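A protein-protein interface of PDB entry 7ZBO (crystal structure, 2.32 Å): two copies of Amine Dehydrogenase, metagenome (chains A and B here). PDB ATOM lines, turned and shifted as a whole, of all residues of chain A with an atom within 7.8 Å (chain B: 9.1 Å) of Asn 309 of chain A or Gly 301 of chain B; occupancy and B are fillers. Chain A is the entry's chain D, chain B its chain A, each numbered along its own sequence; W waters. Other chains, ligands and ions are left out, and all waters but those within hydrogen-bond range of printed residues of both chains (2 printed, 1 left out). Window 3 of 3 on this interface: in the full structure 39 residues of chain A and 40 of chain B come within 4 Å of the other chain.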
ATOM      1  N   PHE A 143     -27.197  -5.451  31.809  1.00  0.00           N
ATOM      2  CA  PHE A 143     -25.752  -5.098  31.765  1.00  0.00           C
ATOM      3  C   PHE A 143     -25.103  -5.485  33.092  1.00  0.00           C
ATOM      4  O   PHE A 143     -23.954  -5.945  33.072  1.00  0.00           O
ATOM      5  CB  PHE A 143     -25.528  -3.617  31.457  1.00  0.00           C
ATOM      6  CG  PHE A 143     -24.088  -3.232  31.207  1.00  0.00           C
ATOM      7  CD1 PHE A 143     -23.515  -3.439  29.962  1.00  0.00           C
ATOM      8  CD2 PHE A 143     -23.306  -2.678  32.214  1.00  0.00           C
ATOM      9  CE1 PHE A 143     -22.190  -3.102  29.721  1.00  0.00           C
ATOM     10  CE2 PHE A 143     -21.985  -2.322  31.966  1.00  0.00           C
ATOM     11  CZ  PHE A 143     -21.425  -2.543  30.728  1.00  0.00           C
ATOM     12  N   GLN A 170     -19.064   3.614  35.557  1.00  0.00           N
ATOM     13  CA  GLN A 170     -19.055   5.082  35.363  1.00  0.00           C
ATOM     14  C   GLN A 170     -19.782   5.369  34.058  1.00  0.00           C
ATOM     15  O   GLN A 170     -19.530   4.660  33.078  1.00  0.00           O
ATOM     16  CB  GLN A 170     -17.638   5.638  35.420  1.00  0.00           C
ATOM     17  CG  GLN A 170     -17.597   7.150  35.278  1.00  0.00           C
ATOM     18  CD  GLN A 170     -16.181   7.686  35.224  1.00  0.00           C
ATOM     19  OE1 GLN A 170     -15.556   7.937  36.252  1.00  0.00           O
ATOM     20  NE2 GLN A 170     -15.681   7.916  34.021  1.00  0.00           N
ATOM     21  N   TYR A 283     -18.380  14.891  33.099  1.00  0.00           N
ATOM     22  CA  TYR A 283     -17.164  14.473  32.340  1.00  0.00           C
ATOM     23  C   TYR A 283     -16.318  15.701  31.985  1.00  0.00           C
ATOM     24  O   TYR A 283     -16.806  16.649  31.335  1.00  0.00           O
ATOM     25  CB  TYR A 283     -17.441  13.637  31.076  1.00  0.00           C
ATOM     26  CG  TYR A 283     -17.783  12.186  31.316  1.00  0.00           C
ATOM     27  CD1 TYR A 283     -18.077  11.722  32.589  1.00  0.00           C
ATOM     28  CD2 TYR A 283     -17.795  11.264  30.278  1.00  0.00           C
ATOM     29  CE1 TYR A 283     -18.396  10.394  32.826  1.00  0.00           C
ATOM     30  CE2 TYR A 283     -18.111   9.928  30.496  1.00  0.00           C
ATOM     31  CZ  TYR A 283     -18.402   9.488  31.780  1.00  0.00           C
ATOM     32  OH  TYR A 283     -18.731   8.190  32.038  1.00  0.00           O
ATOM     33  N   GLY A 286     -10.971  13.497  28.985  1.00  0.00           N
ATOM     34  CA  GLY A 286     -10.345  12.202  29.316  1.00  0.00           C
ATOM     35  C   GLY A 286     -11.276  11.229  30.030  1.00  0.00           C
ATOM     36  O   GLY A 286     -10.924  10.042  30.086  1.00  0.00           O
ATOM     37  N   ASP A 287     -12.395  11.693  30.595  1.00  0.00           N
ATOM     38  CA  ASP A 287     -13.396  10.818  31.270  1.00  0.00           C
ATOM     39  C   ASP A 287     -14.122   9.985  30.209  1.00  0.00           C
ATOM     40  O   ASP A 287     -14.495  10.556  29.172  1.00  0.00           O
ATOM     41  CB  ASP A 287     -14.374  11.626  32.128  1.00  0.00           C
ATOM     42  CG  ASP A 287     -13.750  12.194  33.401  1.00  0.00           C
ATOM     43  OD1 ASP A 287     -12.847  11.542  33.952  1.00  0.00           O
ATOM     44  OD2 ASP A 287     -14.170  13.292  33.842  1.00  0.00           O
ATOM     45  N   GLU A 288     -14.287   8.683  30.449  1.00  0.00           N
ATOM     46  CA  GLU A 288     -15.059   7.771  29.553  1.00  0.00           C
ATOM     47  C   GLU A 288     -15.936   6.848  30.388  1.00  0.00           C
ATOM     48  O   GLU A 288     -15.603   6.615  31.574  1.00  0.00           O
ATOM     49  CB  GLU A 288     -14.202   6.930  28.595  1.00  0.00           C
ATOM     50  CG  GLU A 288     -12.737   6.789  28.927  1.00  0.00           C
ATOM     51  CD  GLU A 288     -11.968   5.958  27.910  1.00  0.00           C
ATOM     52  OE1 GLU A 288     -12.586   5.343  26.989  1.00  0.00           O
ATOM     53  OE2 GLU A 288     -10.744   5.918  28.046  1.00  0.00           O
ATOM     54  N   ASP A 289     -17.024   6.361  29.785  1.00  0.00           N
ATOM     55  CA  ASP A 289     -17.846   5.257  30.351  1.00  0.00           C
ATOM     56  C   ASP A 289     -16.910   4.078  30.617  1.00  0.00           C
ATOM     57  O   ASP A 289     -15.978   3.898  29.824  1.00  0.00           O
ATOM     58  CB  ASP A 289     -18.988   4.836  29.426  1.00  0.00           C
ATOM     59  CG  ASP A 289     -20.088   5.863  29.295  1.00  0.00           C
ATOM     60  OD1 ASP A 289     -19.902   7.026  29.774  1.00  0.00           O
ATOM     61  OD2 ASP A 289     -21.100   5.488  28.667  1.00  0.00           O
ATOM     62  N   MET A 290     -17.126   3.361  31.721  1.00  0.00           N
ATOM     63  CA  MET A 290     -16.135   2.403  32.261  1.00  0.00           C
ATOM     64  C   MET A 290     -16.856   1.352  33.107  1.00  0.00           C
ATOM     65  O   MET A 290     -17.848   1.686  33.773  1.00  0.00           O
ATOM     66  CB  MET A 290     -15.088   3.111  33.124  1.00  0.00           C
ATOM     67  CG  MET A 290     -13.715   2.501  33.032  1.00  0.00           C
ATOM     68  SD  MET A 290     -12.599   3.233  34.242  1.00  0.00           S
ATOM     69  CE  MET A 290     -12.300   4.842  33.509  1.00  0.00           C
ATOM     70  N   VAL A 291     -16.381   0.112  33.020  1.00  0.00           N
ATOM     71  CA  VAL A 291     -16.618  -0.945  34.035  1.00  0.00           C
ATOM     72  C   VAL A 291     -15.233  -1.328  34.549  1.00  0.00           C
ATOM     73  O   VAL A 291     -14.306  -1.413  33.720  1.00  0.00           O
ATOM     74  CB  VAL A 291     -17.342  -2.157  33.433  1.00  0.00           C
ATOM     75  CG1 VAL A 291     -17.506  -3.267  34.461  1.00  0.00           C
ATOM     76  CG2 VAL A 291     -18.671  -1.750  32.787  1.00  0.00           C
ATOM     77  N   THR A 306     -10.735  -4.075  33.178  1.00  0.00           N
ATOM     78  CA  THR A 306     -11.427  -2.811  32.836  1.00  0.00           C
ATOM     79  C   THR A 306     -12.062  -2.986  31.456  1.00  0.00           C
ATOM     80  O   THR A 306     -11.426  -3.640  30.602  1.00  0.00           O
ATOM     81  CB  THR A 306     -10.418  -1.649  32.872  1.00  0.00           C
ATOM     82  OG1 THR A 306      -9.823  -1.584  34.173  1.00  0.00           O
ATOM     83  CG2 THR A 306     -11.052  -0.320  32.533  1.00  0.00           C
ATOM     84  N   MET A 307     -13.260  -2.449  31.243  1.00  0.00           N
ATOM     85  CA  MET A 307     -13.872  -2.265  29.900  1.00  0.00           C
ATOM     86  C   MET A 307     -14.004  -0.754  29.690  1.00  0.00           C
ATOM     87  O   MET A 307     -14.730  -0.117  30.478  1.00  0.00           O
ATOM     88  CB  MET A 307     -15.272  -2.885  29.790  1.00  0.00           C
ATOM     89  CG  MET A 307     -15.336  -4.390  29.875  1.00  0.00           C
ATOM     90  SD  MET A 307     -17.089  -4.931  29.826  1.00  0.00           S
ATOM     91  CE  MET A 307     -16.859  -6.571  29.157  1.00  0.00           C
ATOM     92  N   LYS A 308     -13.321  -0.184  28.697  1.00  0.00           N
ATOM     93  CA  LYS A 308     -13.461   1.251  28.350  1.00  0.00           C
ATOM     94  C   LYS A 308     -14.516   1.382  27.238  1.00  0.00           C
ATOM     95  O   LYS A 308     -14.530   0.544  26.315  1.00  0.00           O
ATOM     96  CB  LYS A 308     -12.098   1.848  27.996  1.00  0.00           C
ATOM     97  CG  LYS A 308     -11.493   2.675  29.122  1.00  0.00           C
ATOM     98  CD  LYS A 308     -10.646   1.882  30.112  1.00  0.00           C
ATOM     99  CE  LYS A 308      -9.154   2.105  29.951  1.00  0.00           C
ATOM    100  NZ  LYS A 308      -8.777   3.540  30.055  1.00  0.00           N
ATOM    101  N   ASN A 309     -15.414   2.347  27.378  1.00  0.00           N
ATOM    102  CA  ASN A 309     -16.391   2.755  26.331  1.00  0.00           C
ATOM    103  C   ASN A 309     -17.260   1.568  25.899  1.00  0.00           C
ATOM    104  O   ASN A 309     -17.521   1.399  24.712  1.00  0.00           O
ATOM    105  CB  ASN A 309     -15.665   3.378  25.131  1.00  0.00           C
ATOM    106  CG  ASN A 309     -16.004   4.834  24.871  1.00  0.00           C
ATOM    107  OD1 ASN A 309     -15.477   5.723  25.539  1.00  0.00           O
ATOM    108  ND2 ASN A 309     -16.845   5.085  23.871  1.00  0.00           N
ATOM    109  N   PRO A 310     -17.761   0.722  26.827  1.00  0.00           N
ATOM    110  CA  PRO A 310     -18.588  -0.420  26.447  1.00  0.00           C
ATOM    111  C   PRO A 310     -19.867   0.054  25.784  1.00  0.00           C
ATOM    112  O   PRO A 310     -20.496   0.975  26.282  1.00  0.00           O
ATOM    113  CB  PRO A 310     -18.912  -1.120  27.776  1.00  0.00           C
ATOM    114  CG  PRO A 310     -18.684  -0.081  28.810  1.00  0.00           C
ATOM    115  CD  PRO A 310     -17.573   0.804  28.281  1.00  0.00           C
ATOM    116  N   PRO A 311     -20.290  -0.526  24.644  1.00  0.00           N
ATOM    117  CA  PRO A 311     -21.615  -0.221  24.090  1.00  0.00           C
ATOM    118  C   PRO A 311     -22.714  -0.831  24.962  1.00  0.00           C
ATOM    119  O   PRO A 311     -23.291  -1.842  24.557  1.00  0.00           O
ATOM    120  CB  PRO A 311     -21.574  -0.862  22.693  1.00  0.00           C
ATOM    121  CG  PRO A 311     -20.583  -1.993  22.843  1.00  0.00           C
ATOM    122  CD  PRO A 311     -19.526  -1.448  23.790  1.00  0.00           C
ATOM    123  N   THR A 312     -23.008  -0.190  26.104  1.00  0.00           N
ATOM    124  CA  THR A 312     -23.870  -0.754  27.180  1.00  0.00           C
ATOM    125  C   THR A 312     -25.270  -1.055  26.648  1.00  0.00           C
ATOM    126  O   THR A 312     -25.820  -2.103  26.967  1.00  0.00           O
ATOM    127  CB  THR A 312     -23.870   0.096  28.468  1.00  0.00           C
ATOM    128  OG1 THR A 312     -24.824   1.135  28.374  1.00  0.00           O
ATOM    129  CG2 THR A 312     -22.536   0.719  28.815  1.00  0.00           C
ATOM    130  N   ALA A 314     -26.505  -1.914  23.617  1.00  0.00           N
ATOM    131  CA  ALA A 314     -26.501  -3.133  22.762  1.00  0.00           C
ATOM    132  C   ALA A 314     -26.128  -4.365  23.614  1.00  0.00           C
ATOM    133  O   ALA A 314     -26.737  -5.458  23.414  1.00  0.00           O
ATOM    134  CB  ALA A 314     -25.547  -2.947  21.592  1.00  0.00           C
ATOM    135  N   MET A 315     -25.186  -4.188  24.550  1.00  0.00           N
ATOM    136  CA  MET A 315     -24.690  -5.301  25.388  1.00  0.00           C
ATOM    137  C   MET A 315     -25.801  -5.759  26.333  1.00  0.00           C
ATOM    138  O   MET A 315     -25.890  -6.987  26.584  1.00  0.00           O
ATOM    139  CB  MET A 315     -23.440  -4.893  26.187  1.00  0.00           C
ATOM    140  CG  MET A 315     -22.192  -4.900  25.326  1.00  0.00           C
ATOM    141  SD  MET A 315     -20.687  -4.648  26.284  1.00  0.00           S
ATOM    142  CE  MET A 315     -20.575  -2.900  26.108  1.00  0.00           C
ATOM    143  N   MET B 159     -21.837 -10.974  22.213  1.00  0.00           N
ATOM    144  CA  MET B 159     -21.776 -10.580  20.792  1.00  0.00           C
ATOM    145  C   MET B 159     -22.911 -11.274  20.021  1.00  0.00           C
ATOM    146  O   MET B 159     -23.185 -12.454  20.294  1.00  0.00           O
ATOM    147  CB  MET B 159     -20.420 -10.952  20.176  1.00  0.00           C
ATOM    148  CG  MET B 159     -19.232 -10.304  20.853  1.00  0.00           C
ATOM    149  SD  MET B 159     -19.259  -8.523  20.761  1.00  0.00           S
ATOM    150  CE  MET B 159     -18.876  -8.275  19.017  1.00  0.00           C
ATOM    151  N   ASN B 294     -10.432  -7.804  22.295  1.00  0.00           N
ATOM    152  CA  ASN B 294     -11.420  -6.856  21.739  1.00  0.00           C
ATOM    153  C   ASN B 294     -12.193  -7.585  20.637  1.00  0.00           C
ATOM    154  O   ASN B 294     -11.585  -8.334  19.884  1.00  0.00           O
ATOM    155  CB  ASN B 294     -10.780  -5.532  21.318  1.00  0.00           C
ATOM    156  CG  ASN B 294     -11.857  -4.500  21.018  1.00  0.00           C
ATOM    157  OD1 ASN B 294     -12.592  -4.064  21.909  1.00  0.00           O
ATOM    158  ND2 ASN B 294     -12.032  -4.124  19.759  1.00  0.00           N
ATOM    159  N   LEU B 295     -13.505  -7.415  20.619  1.00  0.00           N
ATOM    160  CA  LEU B 295     -14.405  -8.086  19.672  1.00  0.00           C
ATOM    161  C   LEU B 295     -15.049  -6.987  18.816  1.00  0.00           C
ATOM    162  O   LEU B 295     -15.574  -6.005  19.366  1.00  0.00           O
ATOM    163  CB  LEU B 295     -15.436  -8.945  20.418  1.00  0.00           C
ATOM    164  CG  LEU B 295     -14.845  -9.901  21.449  1.00  0.00           C
ATOM    165  CD1 LEU B 295     -15.928 -10.509  22.346  1.00  0.00           C
ATOM    166  CD2 LEU B 295     -14.044 -11.015  20.779  1.00  0.00           C
ATOM    167  N   GLU B 296     -14.934  -7.143  17.498  1.00  0.00           N
ATOM    168  CA  GLU B 296     -15.529  -6.253  16.503  1.00  0.00           C
ATOM    169  C   GLU B 296     -16.662  -7.019  15.827  1.00  0.00           C
ATOM    170  O   GLU B 296     -16.478  -8.213  15.517  1.00  0.00           O
ATOM    171  CB  GLU B 296     -14.419  -5.810  15.564  1.00  0.00           C
ATOM    172  CG  GLU B 296     -14.371  -4.329  15.413  1.00  0.00           C
ATOM    173  CD  GLU B 296     -13.862  -3.537  16.581  1.00  0.00           C
ATOM    174  OE1 GLU B 296     -12.747  -3.814  17.011  1.00  0.00           O
ATOM    175  OE2 GLU B 296     -14.583  -2.626  16.995  1.00  0.00           O
ATOM    176  N   GLY B 297     -17.769  -6.337  15.580  1.00  0.00           N
ATOM    177  CA  GLY B 297     -18.948  -6.905  14.897  1.00  0.00           C
ATOM    178  C   GLY B 297     -20.218  -6.173  15.285  1.00  0.00           C
ATOM    179  O   GLY B 297     -20.273  -4.982  15.052  1.00  0.00           O
ATOM    180  N   ASN B 298     -21.150  -6.866  15.931  1.00  0.00           N
ATOM    181  CA  ASN B 298     -22.383  -6.302  16.523  1.00  0.00           C
ATOM    182  C   ASN B 298     -22.605  -6.981  17.866  1.00  0.00           C
ATOM    183  O   ASN B 298     -22.811  -8.190  17.871  1.00  0.00           O
ATOM    184  CB  ASN B 298     -23.568  -6.505  15.581  1.00  0.00           C
ATOM    185  CG  ASN B 298     -24.830  -5.792  16.022  1.00  0.00           C
ATOM    186  OD1 ASN B 298     -24.870  -5.119  17.052  1.00  0.00           O
ATOM    187  ND2 ASN B 298     -25.871  -5.905  15.226  1.00  0.00           N
ATOM    188  N   PRO B 299     -22.607  -6.284  19.028  1.00  0.00           N
ATOM    189  CA  PRO B 299     -22.438  -4.822  19.126  1.00  0.00           C
ATOM    190  C   PRO B 299     -21.233  -4.170  18.424  1.00  0.00           C
ATOM    191  O   PRO B 299     -20.178  -4.769  18.384  1.00  0.00           O
ATOM    192  CB  PRO B 299     -22.271  -4.581  20.643  1.00  0.00           C
ATOM    193  CG  PRO B 299     -23.030  -5.744  21.278  1.00  0.00           C
ATOM    194  CD  PRO B 299     -22.851  -6.914  20.333  1.00  0.00           C
ATOM    195  N   THR B 300     -21.416  -2.956  17.909  1.00  0.00           N
ATOM    196  CA  THR B 300     -20.457  -2.311  16.980  1.00  0.00           C
ATOM    197  C   THR B 300     -19.407  -1.456  17.703  1.00  0.00           C
ATOM    198  O   THR B 300     -18.319  -1.321  17.103  1.00  0.00           O
ATOM    199  CB  THR B 300     -21.170  -1.466  15.919  1.00  0.00           C
ATOM    200  OG1 THR B 300     -21.796  -0.346  16.550  1.00  0.00           O
ATOM    201  CG2 THR B 300     -22.193  -2.261  15.140  1.00  0.00           C
ATOM    202  N   GLY B 301     -19.671  -0.953  18.913  1.00  0.00           N
ATOM    203  CA  GLY B 301     -18.872   0.134  19.505  1.00  0.00           C
ATOM    204  C   GLY B 301     -17.623  -0.328  20.239  1.00  0.00           C
ATOM    205  O   GLY B 301     -16.984   0.511  20.876  1.00  0.00           O
ATOM    206  N   GLY B 302     -17.268  -1.603  20.143  1.00  0.00           N
ATOM    207  CA  GLY B 302     -15.985  -2.159  20.624  1.00  0.00           C
ATOM    208  C   GLY B 302     -16.120  -2.829  21.982  1.00  0.00           C
ATOM    209  O   GLY B 302     -16.051  -2.073  22.968  1.00  0.00           O
ATOM    210  N   VAL B 303     -16.294  -4.155  22.004  1.00  0.00           N
ATOM    211  CA  VAL B 303     -16.539  -4.977  23.210  1.00  0.00           C
ATOM    212  C   VAL B 303     -15.220  -5.628  23.609  1.00  0.00           C
ATOM    213  O   VAL B 303     -14.858  -6.641  23.016  1.00  0.00           O
ATOM    214  CB  VAL B 303     -17.605  -6.047  22.929  1.00  0.00           C
ATOM    215  CG1 VAL B 303     -17.848  -6.934  24.136  1.00  0.00           C
ATOM    216  CG2 VAL B 303     -18.887  -5.421  22.441  1.00  0.00           C
ATOM    217  N   GLY B 304     -14.547  -5.080  24.616  1.00  0.00           N
ATOM    218  CA  GLY B 304     -13.199  -5.535  24.986  1.00  0.00           C
ATOM    219  C   GLY B 304     -12.955  -5.386  26.464  1.00  0.00           C
ATOM    220  O   GLY B 304     -13.633  -4.562  27.107  1.00  0.00           O
HETATM  221  O   HOH W   1     -18.699   2.392  22.348  1.00  0.00           O
HETATM  222  O   HOH W   2     -15.583  -1.889  25.678  1.00  0.00           O
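Among the printed residues, merely in contact across the chains: Met 307 of chain A with Gly 304 of chain B, Pro 311 of chain A with Gly 302 of chain B, Ala 314 of chain A with Pro 299 of chain B, Pro 311 of chain A with Pro 299 of chain B, Pro 311 of chain A with Val 303 of chain B and Asn 309 of chain A with Gly 301 of chain B.
Asn 309 of chain A touches one residue of chain B.
Of chain A, only Asn 309 comes within 4 Å of Gly 301 of chain B.
No residue of chain B comes within 4 Å of Pro 310 of chain A.
Gly 302 of chain B touches one residue of chain A.
Of the printed residues of chain A, Val 303 of chain B touches Pro 311.
Of the printed residues of chain A, Gly 304 of chain B touches Met 307.
Of the printed residues of chain B, Met 307 of chain A touches Gly 304 (3.3 Å).
Of the printed residues of chain B, Pro 311 of chain A touches Pro 299 (3.8 Å), Gly 302 (3.6 Å) and Val 303 (3.8 Å).
Printed residues of chain B within 4 Å of Ala 314 of chain A: Pro 299 (3.8 Å).
Gly 286 of chain A touches none of the printed residues of chain B.
Gln 170 of chain A touches none of the printed residues of chain B.
The nearest residue of chain B that does not touch Asn 309 of chain A is Gly 302 of chain B (4.2 Å).
The nearest printed residue of chain B that does not touch Pro 311 of chain A is Gly 301 of chain B (4.2 Å).
Water W2 bridges O of Lys 308 of chain A (2.7 Å) and O of Gly 302 of chain B (2.8 Å).
Water W1 bridges O of Asn 309 of chain A (2.8 Å) and O of Gly 301 of chain B (2.9 Å).
Printed residues of chain A that touch a printed residue of chain B: Met 307, Asn 309, Pro 311 and Ala 314.
Hydrophobic or aromatic side chains of chain A within 4 Å of the printed part of chain B: Met 307, Pro 311 and Ala 314.
Of the 12 printed residues of chain B, 5 touch a printed residue of chain A.
Hydrophobic or aromatic side chains of chain B within 4 Å of the printed part of chain A: Pro 299 and Val 303.
N of Gly 304 of chain B lies close to OD1 of Asn 294 of chain B, 3.5 Å away.
OE1 of Glu 288 of chain A lies close to OD1 of Asn 309 of chain A, 3.3 Å away.
The backbone NH (N) of Leu 295 of chain B is in hydrogen-bond range of the backbone carbonyl oxygen (O) of Val 303 of chain B, at 2.9 Å.
N of Asn 309 of chain A is in hydrogen-bond range of O of Asp 289 of chain A.
The backbone carbonyl oxygen of Val 291 of chain A sits at hydrogen-bond distance from the backbone NH of Met 307 of chain A.
No position is printed for both chains.
Of the 6 pairs that touch across the chains among the printed residues, none has its exchanged pair printed and touching as well.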
